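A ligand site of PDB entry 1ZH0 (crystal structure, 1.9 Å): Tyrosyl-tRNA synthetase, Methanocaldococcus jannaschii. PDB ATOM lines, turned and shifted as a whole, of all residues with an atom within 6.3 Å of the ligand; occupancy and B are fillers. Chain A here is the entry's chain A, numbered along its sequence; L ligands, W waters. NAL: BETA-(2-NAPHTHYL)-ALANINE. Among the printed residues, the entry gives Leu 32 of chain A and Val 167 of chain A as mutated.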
ATOM      1  N   LEU A  32     -13.579  -7.014  19.861  1.00  0.00           N
ATOM      2  CA  LEU A  32     -12.842  -6.845  21.118  1.00  0.00           C
ATOM      3  C   LEU A  32     -12.904  -5.428  21.636  1.00  0.00           C
ATOM      4  O   LEU A  32     -12.770  -4.469  20.869  1.00  0.00           O
ATOM      5  CB  LEU A  32     -11.369  -7.190  20.877  1.00  0.00           C
ATOM      6  CG  LEU A  32     -10.355  -6.879  21.970  1.00  0.00           C
ATOM      7  CD1 LEU A  32     -10.392  -8.044  22.907  1.00  0.00           C
ATOM      8  CD2 LEU A  32      -8.960  -6.735  21.380  1.00  0.00           C
ATOM      9  N   ILE A  33     -13.005  -5.246  22.964  1.00  0.00           N
ATOM     10  CA  ILE A  33     -12.646  -3.942  23.566  1.00  0.00           C
ATOM     11  C   ILE A  33     -11.829  -4.241  24.777  1.00  0.00           C
ATOM     12  O   ILE A  33     -12.032  -5.313  25.406  1.00  0.00           O
ATOM     13  CB  ILE A  33     -13.885  -3.106  23.958  1.00  0.00           C
ATOM     14  CG1 ILE A  33     -13.480  -1.746  24.549  1.00  0.00           C
ATOM     15  CG2 ILE A  33     -14.812  -3.884  24.868  1.00  0.00           C
ATOM     16  CD1 ILE A  33     -14.581  -0.782  24.464  1.00  0.00           C
ATOM     17  N   GLY A  34     -10.879  -3.361  25.080  1.00  0.00           N
ATOM     18  CA  GLY A  34     -10.072  -3.503  26.263  1.00  0.00           C
ATOM     19  C   GLY A  34     -10.314  -2.365  27.201  1.00  0.00           C
ATOM     20  O   GLY A  34     -10.452  -1.247  26.782  1.00  0.00           O
ATOM     21  N   PHE A  35     -10.284  -2.640  28.500  1.00  0.00           N
ATOM     22  CA  PHE A  35     -10.426  -1.578  29.498  1.00  0.00           C
ATOM     23  C   PHE A  35      -9.369  -1.733  30.562  1.00  0.00           C
ATOM     24  O   PHE A  35      -9.285  -2.804  31.164  1.00  0.00           O
ATOM     25  CB  PHE A  35     -11.744  -1.722  30.250  1.00  0.00           C
ATOM     26  CG  PHE A  35     -12.963  -1.369  29.458  1.00  0.00           C
ATOM     27  CD1 PHE A  35     -13.850  -2.343  29.064  1.00  0.00           C
ATOM     28  CD2 PHE A  35     -13.221  -0.067  29.132  1.00  0.00           C
ATOM     29  CE1 PHE A  35     -14.954  -2.024  28.336  1.00  0.00           C
ATOM     30  CE2 PHE A  35     -14.377   0.272  28.427  1.00  0.00           C
ATOM     31  CZ  PHE A  35     -15.231  -0.708  28.030  1.00  0.00           C
ATOM     32  N   GLU A  36      -8.618  -0.658  30.847  1.00  0.00           N
ATOM     33  CA  GLU A  36      -7.868  -0.622  32.108  1.00  0.00           C
ATOM     34  C   GLU A  36      -8.916  -0.790  33.186  1.00  0.00           C
ATOM     35  O   GLU A  36      -9.853  -0.018  33.218  1.00  0.00           O
ATOM     36  CB  GLU A  36      -7.165   0.738  32.284  1.00  0.00           C
ATOM     37  CG  GLU A  36      -5.852   0.853  31.497  1.00  0.00           C
ATOM     38  CD  GLU A  36      -5.119   2.144  31.754  1.00  0.00           C
ATOM     39  OE1 GLU A  36      -5.057   2.550  32.909  1.00  0.00           O
ATOM     40  OE2 GLU A  36      -4.603   2.741  30.792  1.00  0.00           O
ATOM     41  N   PRO A  37      -8.835  -1.824  34.040  1.00  0.00           N
ATOM     42  CA  PRO A  37      -9.907  -1.887  35.013  1.00  0.00           C
ATOM     43  C   PRO A  37     -10.063  -0.594  35.843  1.00  0.00           C
ATOM     44  O   PRO A  37      -9.059  -0.006  36.328  1.00  0.00           O
ATOM     45  CB  PRO A  37      -9.491  -3.049  35.916  1.00  0.00           C
ATOM     46  CG  PRO A  37      -8.712  -3.914  35.073  1.00  0.00           C
ATOM     47  CD  PRO A  37      -7.927  -2.967  34.170  1.00  0.00           C
ATOM     48  N   LEU A  65     -11.234  -7.505  26.983  1.00  0.00           N
ATOM     49  CA  LEU A  65      -9.946  -7.667  27.624  1.00  0.00           C
ATOM     50  C   LEU A  65      -9.899  -6.800  28.876  1.00  0.00           C
ATOM     51  O   LEU A  65     -10.076  -5.574  28.811  1.00  0.00           O
ATOM     52  CB  LEU A  65      -8.782  -7.284  26.711  1.00  0.00           C
ATOM     53  CG  LEU A  65      -7.439  -7.095  27.356  1.00  0.00           C
ATOM     54  CD1 LEU A  65      -6.761  -8.396  27.754  1.00  0.00           C
ATOM     55  CD2 LEU A  65      -6.625  -6.293  26.373  1.00  0.00           C
ATOM     56  N   ALA A  67      -7.581  -5.260  31.090  1.00  0.00           N
ATOM     57  CA  ALA A  67      -6.210  -4.924  30.742  1.00  0.00           C
ATOM     58  C   ALA A  67      -5.473  -4.547  31.984  1.00  0.00           C
ATOM     59  O   ALA A  67      -5.065  -3.406  32.155  1.00  0.00           O
ATOM     60  CB  ALA A  67      -6.185  -3.775  29.754  1.00  0.00           C
ATOM     61  N   HIS A  70      -1.677  -3.448  31.384  1.00  0.00           N
ATOM     62  CA  HIS A  70      -1.653  -2.094  30.884  1.00  0.00           C
ATOM     63  C   HIS A  70      -1.944  -1.065  31.967  1.00  0.00           C
ATOM     64  O   HIS A  70      -1.335   0.035  32.054  1.00  0.00           O
ATOM     65  CB  HIS A  70      -2.631  -1.953  29.779  1.00  0.00           C
ATOM     66  CG  HIS A  70      -2.073  -2.296  28.440  1.00  0.00           C
ATOM     67  ND1 HIS A  70      -2.143  -3.570  27.917  1.00  0.00           N
ATOM     68  CD2 HIS A  70      -1.472  -1.526  27.497  1.00  0.00           C
ATOM     69  CE1 HIS A  70      -1.601  -3.562  26.704  1.00  0.00           C
ATOM     70  NE2 HIS A  70      -1.192  -2.345  26.434  1.00  0.00           N
ATOM     71  N   ASN A  74       0.324   1.799  33.342  1.00  0.00           N
ATOM     72  CA  ASN A  74      -0.219   3.159  33.367  1.00  0.00           C
ATOM     73  C   ASN A  74      -0.519   3.612  34.797  1.00  0.00           C
ATOM     74  O   ASN A  74      -1.423   4.440  35.012  1.00  0.00           O
ATOM     75  CB  ASN A  74      -1.423   3.255  32.406  1.00  0.00           C
ATOM     76  CG  ASN A  74      -1.685   4.665  31.927  1.00  0.00           C
ATOM     77  OD1 ASN A  74      -2.766   4.974  31.414  1.00  0.00           O
ATOM     78  ND2 ASN A  74      -0.728   5.551  32.123  1.00  0.00           N
ATOM     79  N   GLN A 109      -0.141 -12.076  28.901  1.00  0.00           N
ATOM     80  CA  GLN A 109       0.764 -11.044  28.462  1.00  0.00           C
ATOM     81  C   GLN A 109       2.171 -11.174  28.988  1.00  0.00           C
ATOM     82  O   GLN A 109       2.986 -10.316  28.736  1.00  0.00           O
ATOM     83  CB  GLN A 109       0.220  -9.673  28.851  1.00  0.00           C
ATOM     84  CG  GLN A 109      -0.955  -9.261  28.024  1.00  0.00           C
ATOM     85  CD  GLN A 109      -1.378  -7.896  28.376  1.00  0.00           C
ATOM     86  OE1 GLN A 109      -1.004  -6.915  27.713  1.00  0.00           O
ATOM     87  NE2 GLN A 109      -2.046  -7.787  29.489  1.00  0.00           N
ATOM     88  N   ILE A 137      -3.927   9.125  26.829  1.00  0.00           N
ATOM     89  CA  ILE A 137      -4.026   7.905  27.634  1.00  0.00           C
ATOM     90  C   ILE A 137      -3.123   7.931  28.855  1.00  0.00           C
ATOM     91  O   ILE A 137      -3.516   7.569  29.983  1.00  0.00           O
ATOM     92  CB  ILE A 137      -3.640   6.713  26.719  1.00  0.00           C
ATOM     93  CG1 ILE A 137      -4.694   6.565  25.642  1.00  0.00           C
ATOM     94  CG2 ILE A 137      -3.554   5.386  27.499  1.00  0.00           C
ATOM     95  CD1 ILE A 137      -4.366   5.470  24.627  1.00  0.00           C
ATOM     96  N   TYR A 151       3.532   0.619  26.996  1.00  0.00           N
ATOM     97  CA  TYR A 151       2.071   0.478  26.916  1.00  0.00           C
ATOM     98  C   TYR A 151       1.506   0.377  25.514  1.00  0.00           C
ATOM     99  O   TYR A 151       0.805  -0.534  25.214  1.00  0.00           O
ATOM    100  CB  TYR A 151       1.421   1.662  27.666  1.00  0.00           C
ATOM    101  CG  TYR A 151      -0.061   1.627  27.834  1.00  0.00           C
ATOM    102  CD1 TYR A 151      -0.631   1.503  29.094  1.00  0.00           C
ATOM    103  CD2 TYR A 151      -0.914   1.859  26.730  1.00  0.00           C
ATOM    104  CE1 TYR A 151      -2.010   1.515  29.250  1.00  0.00           C
ATOM    105  CE2 TYR A 151      -2.293   1.848  26.879  1.00  0.00           C
ATOM    106  CZ  TYR A 151      -2.825   1.664  28.130  1.00  0.00           C
ATOM    107  OH  TYR A 151      -4.174   1.698  28.305  1.00  0.00           O
ATOM    108  N   MET A 154       2.600  -2.813  23.669  1.00  0.00           N
ATOM    109  CA  MET A 154       1.863  -3.935  24.186  1.00  0.00           C
ATOM    110  C   MET A 154       0.468  -3.958  23.634  1.00  0.00           C
ATOM    111  O   MET A 154      -0.042  -5.012  23.316  1.00  0.00           O
ATOM    112  CB  MET A 154       1.801  -3.927  25.694  1.00  0.00           C
ATOM    113  CG  MET A 154       2.978  -4.617  26.379  1.00  0.00           C
ATOM    114  SD  MET A 154       2.710  -4.510  28.173  1.00  0.00           S
ATOM    115  CE  MET A 154       2.897  -6.171  28.685  1.00  0.00           C
ATOM    116  N   GLN A 155      -0.150  -2.800  23.475  1.00  0.00           N
ATOM    117  CA  GLN A 155      -1.571  -2.777  23.054  1.00  0.00           C
ATOM    118  C   GLN A 155      -1.752  -3.191  21.595  1.00  0.00           C
ATOM    119  O   GLN A 155      -2.863  -3.573  21.175  1.00  0.00           O
ATOM    120  CB  GLN A 155      -2.195  -1.429  23.344  1.00  0.00           C
ATOM    121  CG  GLN A 155      -3.595  -1.248  22.749  1.00  0.00           C
ATOM    122  CD  GLN A 155      -4.369  -0.081  23.327  1.00  0.00           C
ATOM    123  OE1 GLN A 155      -4.122   0.374  24.466  1.00  0.00           O
ATOM    124  NE2 GLN A 155      -5.366   0.387  22.547  1.00  0.00           N
ATOM    125  N   VAL A 156      -0.644  -3.186  20.861  1.00  0.00           N
ATOM    126  CA  VAL A 156      -0.565  -3.484  19.415  1.00  0.00           C
ATOM    127  C   VAL A 156      -0.067  -4.944  19.227  1.00  0.00           C
ATOM    128  O   VAL A 156       0.156  -5.408  18.145  1.00  0.00           O
ATOM    129  CB  VAL A 156       0.267  -2.335  18.883  1.00  0.00           C
ATOM    130  CG1 VAL A 156       1.399  -2.711  17.953  1.00  0.00           C
ATOM    131  CG2 VAL A 156      -0.666  -1.187  18.439  1.00  0.00           C
ATOM    132  N   HIS A 160      -3.496  -9.911  20.855  1.00  0.00           N
ATOM    133  CA  HIS A 160      -4.779  -9.308  21.148  1.00  0.00           C
ATOM    134  C   HIS A 160      -5.780  -9.369  20.002  1.00  0.00           C
ATOM    135  O   HIS A 160      -7.001  -9.284  20.241  1.00  0.00           O
ATOM    136  CB  HIS A 160      -4.617  -7.889  21.595  1.00  0.00           C
ATOM    137  CG  HIS A 160      -3.939  -7.781  22.904  1.00  0.00           C
ATOM    138  ND1 HIS A 160      -2.819  -7.001  23.098  1.00  0.00           N
ATOM    139  CD2 HIS A 160      -4.158  -8.408  24.082  1.00  0.00           C
ATOM    140  CE1 HIS A 160      -2.398  -7.137  24.339  1.00  0.00           C
ATOM    141  NE2 HIS A 160      -3.188  -7.972  24.970  1.00  0.00           N
ATOM    142  N   TYR A 161      -5.282  -9.503  18.782  1.00  0.00           N
ATOM    143  CA  TYR A 161      -6.122  -9.358  17.585  1.00  0.00           C
ATOM    144  C   TYR A 161      -6.331 -10.667  16.894  1.00  0.00           C
ATOM    145  O   TYR A 161      -7.011 -10.713  15.885  1.00  0.00           O
ATOM    146  CB  TYR A 161      -5.503  -8.320  16.646  1.00  0.00           C
ATOM    147  CG  TYR A 161      -5.299  -6.995  17.339  1.00  0.00           C
ATOM    148  CD1 TYR A 161      -4.162  -6.754  18.079  1.00  0.00           C
ATOM    149  CD2 TYR A 161      -6.288  -6.014  17.348  1.00  0.00           C
ATOM    150  CE1 TYR A 161      -3.974  -5.562  18.788  1.00  0.00           C
ATOM    151  CE2 TYR A 161      -6.093  -4.801  18.059  1.00  0.00           C
ATOM    152  CZ  TYR A 161      -4.948  -4.604  18.773  1.00  0.00           C
ATOM    153  OH  TYR A 161      -4.776  -3.398  19.431  1.00  0.00           O
ATOM    154  N   VAL A 167     -12.083  -4.057  16.539  1.00  0.00           N
ATOM    155  CA  VAL A 167     -11.741  -3.550  17.865  1.00  0.00           C
ATOM    156  C   VAL A 167     -12.453  -2.232  18.124  1.00  0.00           C
ATOM    157  O   VAL A 167     -12.603  -1.400  17.234  1.00  0.00           O
ATOM    158  CB  VAL A 167     -10.170  -3.358  18.098  1.00  0.00           C
ATOM    159  CG1 VAL A 167      -9.395  -4.612  17.774  1.00  0.00           C
ATOM    160  CG2 VAL A 167      -9.685  -2.186  17.350  1.00  0.00           C
ATOM    161  N   VAL A 168     -12.985  -2.110  19.333  1.00  0.00           N
ATOM    162  CA  VAL A 168     -13.753  -0.941  19.746  1.00  0.00           C
ATOM    163  C   VAL A 168     -13.011  -0.243  20.849  1.00  0.00           C
ATOM    164  O   VAL A 168     -12.393  -0.877  21.700  1.00  0.00           O
ATOM    165  CB  VAL A 168     -15.197  -1.366  20.211  1.00  0.00           C
ATOM    166  CG1 VAL A 168     -16.061  -0.190  20.584  1.00  0.00           C
ATOM    167  CG2 VAL A 168     -15.889  -2.204  19.175  1.00  0.00           C
ATOM    168  N   GLU A 172      -9.760   8.379  22.123  1.00  0.00           N
ATOM    169  CA  GLU A 172      -8.417   8.536  22.687  1.00  0.00           C
ATOM    170  C   GLU A 172      -7.456   7.384  22.324  1.00  0.00           C
ATOM    171  O   GLU A 172      -6.234   7.586  22.342  1.00  0.00           O
ATOM    172  CB  GLU A 172      -8.441   8.820  24.208  1.00  0.00           C
ATOM    173  CG  GLU A 172      -8.598   7.600  25.077  1.00  0.00           C
ATOM    174  CD  GLU A 172      -9.994   6.963  25.015  1.00  0.00           C
ATOM    175  OE1 GLU A 172     -10.112   5.805  25.470  1.00  0.00           O
ATOM    176  OE2 GLU A 172     -10.963   7.615  24.546  1.00  0.00           O
ATOM    177  N   GLN A 173      -8.011   6.210  21.989  1.00  0.00           N
ATOM    178  CA  GLN A 173      -7.269   5.056  21.490  1.00  0.00           C
ATOM    179  C   GLN A 173      -6.876   5.120  20.012  1.00  0.00           C
ATOM    180  O   GLN A 173      -6.148   4.244  19.577  1.00  0.00           O
ATOM    181  CB  GLN A 173      -8.125   3.796  21.607  1.00  0.00           C
ATOM    182  CG  GLN A 173      -8.754   3.508  22.983  1.00  0.00           C
ATOM    183  CD  GLN A 173      -7.747   3.403  24.041  1.00  0.00           C
ATOM    184  OE1 GLN A 173      -6.788   2.605  23.939  1.00  0.00           O
ATOM    185  NE2 GLN A 173      -7.925   4.175  25.093  1.00  0.00           N
ATOM    186  N   ILE A 176      -3.130   4.668  18.837  1.00  0.00           N
ATOM    187  CA  ILE A 176      -2.659   3.316  19.080  1.00  0.00           C
ATOM    188  C   ILE A 176      -3.274   2.360  18.065  1.00  0.00           C
ATOM    189  O   ILE A 176      -2.589   1.488  17.539  1.00  0.00           O
ATOM    190  CB  ILE A 176      -2.964   2.806  20.513  1.00  0.00           C
ATOM    191  CG1 ILE A 176      -2.190   3.592  21.569  1.00  0.00           C
ATOM    192  CG2 ILE A 176      -2.661   1.302  20.636  1.00  0.00           C
ATOM    193  CD1 ILE A 176      -2.664   3.351  22.940  1.00  0.00           C
ATOM    194  N   HIS A 177      -4.596   2.468  17.842  1.00  0.00           N
ATOM    195  CA  HIS A 177      -5.262   1.623  16.831  1.00  0.00           C
ATOM    196  C   HIS A 177      -4.654   1.811  15.446  1.00  0.00           C
ATOM    197  O   HIS A 177      -4.516   0.830  14.696  1.00  0.00           O
ATOM    198  CB  HIS A 177      -6.774   1.832  16.781  1.00  0.00           C
ATOM    199  CG  HIS A 177      -7.494   1.327  17.994  1.00  0.00           C
ATOM    200  ND1 HIS A 177      -8.791   1.692  18.295  1.00  0.00           N
ATOM    201  CD2 HIS A 177      -7.089   0.515  18.994  1.00  0.00           C
ATOM    202  CE1 HIS A 177      -9.144   1.131  19.443  1.00  0.00           C
ATOM    203  NE2 HIS A 177      -8.146   0.361  19.856  1.00  0.00           N
HETATM  204  C1  NAL L   1      -7.251  -1.654  25.101  1.00  0.00           C
HETATM  205  C2  NAL L   1      -6.463  -1.497  26.232  1.00  0.00           C
HETATM  206  C3  NAL L   1      -5.310  -2.291  26.401  1.00  0.00           C
HETATM  207  C4  NAL L   1      -4.978  -3.266  25.473  1.00  0.00           C
HETATM  208  C4A NAL L   1      -5.794  -3.446  24.346  1.00  0.00           C
HETATM  209  C5  NAL L   1      -5.467  -4.379  23.374  1.00  0.00           C
HETATM  210  C6  NAL L   1      -6.250  -4.504  22.254  1.00  0.00           C
HETATM  211  C7  NAL L   1      -7.381  -3.731  22.072  1.00  0.00           C
HETATM  212  C8  NAL L   1      -7.714  -2.787  23.031  1.00  0.00           C
HETATM  213  C8A NAL L   1      -6.924  -2.636  24.169  1.00  0.00           C
HETATM  214  C9  NAL L   1      -6.907  -0.545  27.321  1.00  0.00           C
HETATM  215  CA  NAL L   1      -7.075   0.845  26.749  1.00  0.00           C
HETATM  216  C   NAL L   1      -7.534   1.823  27.879  1.00  0.00           C
HETATM  217  N   NAL L   1      -5.786   1.304  26.195  1.00  0.00           N
HETATM  218  O   NAL L   1      -7.195   3.027  27.775  1.00  0.00           O
HETATM  219  OXT NAL L   1      -8.350   1.463  28.774  1.00  0.00           O
HETATM  220  O   HOH W   1     -10.233  -0.837  23.081  1.00  0.00           O
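The side-chain amide oxygen (OE1) of Gln 155 lies within hydrogen-bond range of a nitrogen (N) of the ligand, 2.6 Å away.
OH of Tyr 151 sits at hydrogen-bond distance from N of the ligand, at 2.7 Å.
N of the ligand is in hydrogen-bond range of OE1 of Gln 173, at 2.8 Å.
OXT of the ligand is in hydrogen-bond range of N of Glu 36, 3.0 Å away.
The backbone carbonyl oxygen (O) of Gln 155 lies within hydrogen-bond range of the side-chain hydroxyl (OH) of Tyr 161.
The backbone NH of Gln 155 is in hydrogen-bond range of a ring nitrogen (NE2) of His 70 (3.2 Å).
The side-chain hydroxyl of Tyr 151 lies within hydrogen-bond range of the side-chain carboxylate of Glu 36.
A ring nitrogen (NE2) of His 70 sits at hydrogen-bond distance from the backbone carbonyl oxygen (O) of Tyr 151, at 3.0 Å.
The side-chain amide nitrogen (NE2) of Gln 173 is in hydrogen-bond range of the side-chain carboxylate (OE1) of Glu 172 (2.8 Å).
The side-chain carboxylate (OE2) of Glu 36 sits close to the side-chain amide oxygen (OD1) of Asn 74 (3.0 Å).
O of Leu 65 lies within hydrogen-bond range of N of Phe 35 (3.0 Å).
The backbone NH (N) of Leu 65 sits at hydrogen-bond distance from the backbone carbonyl oxygen (O) of Ile 33 (2.8 Å).
Merely in contact with the ligand: Leu 32, Gly 34, Phe 35, Leu 65, Ala 67, His 70, His 160 and Tyr 161.
Hydrophobic or aromatic side chains that line the ligand: Leu 32, Leu 65, Ala 67, His 70, Tyr 151, His 160 and Tyr 161.
Within 4 Å of the ligand: Leu 32, Gly 34, Phe 35, Glu 36, Leu 65, Ala 67, His 70, Tyr 151, Gln 155, His 160, Tyr 161 and Gln 173.
The nearest printed residue that does not touch the ligand is Ile 137 (4.3 Å).
Water W1 bridges O of Val 168 and N of Gly 34.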
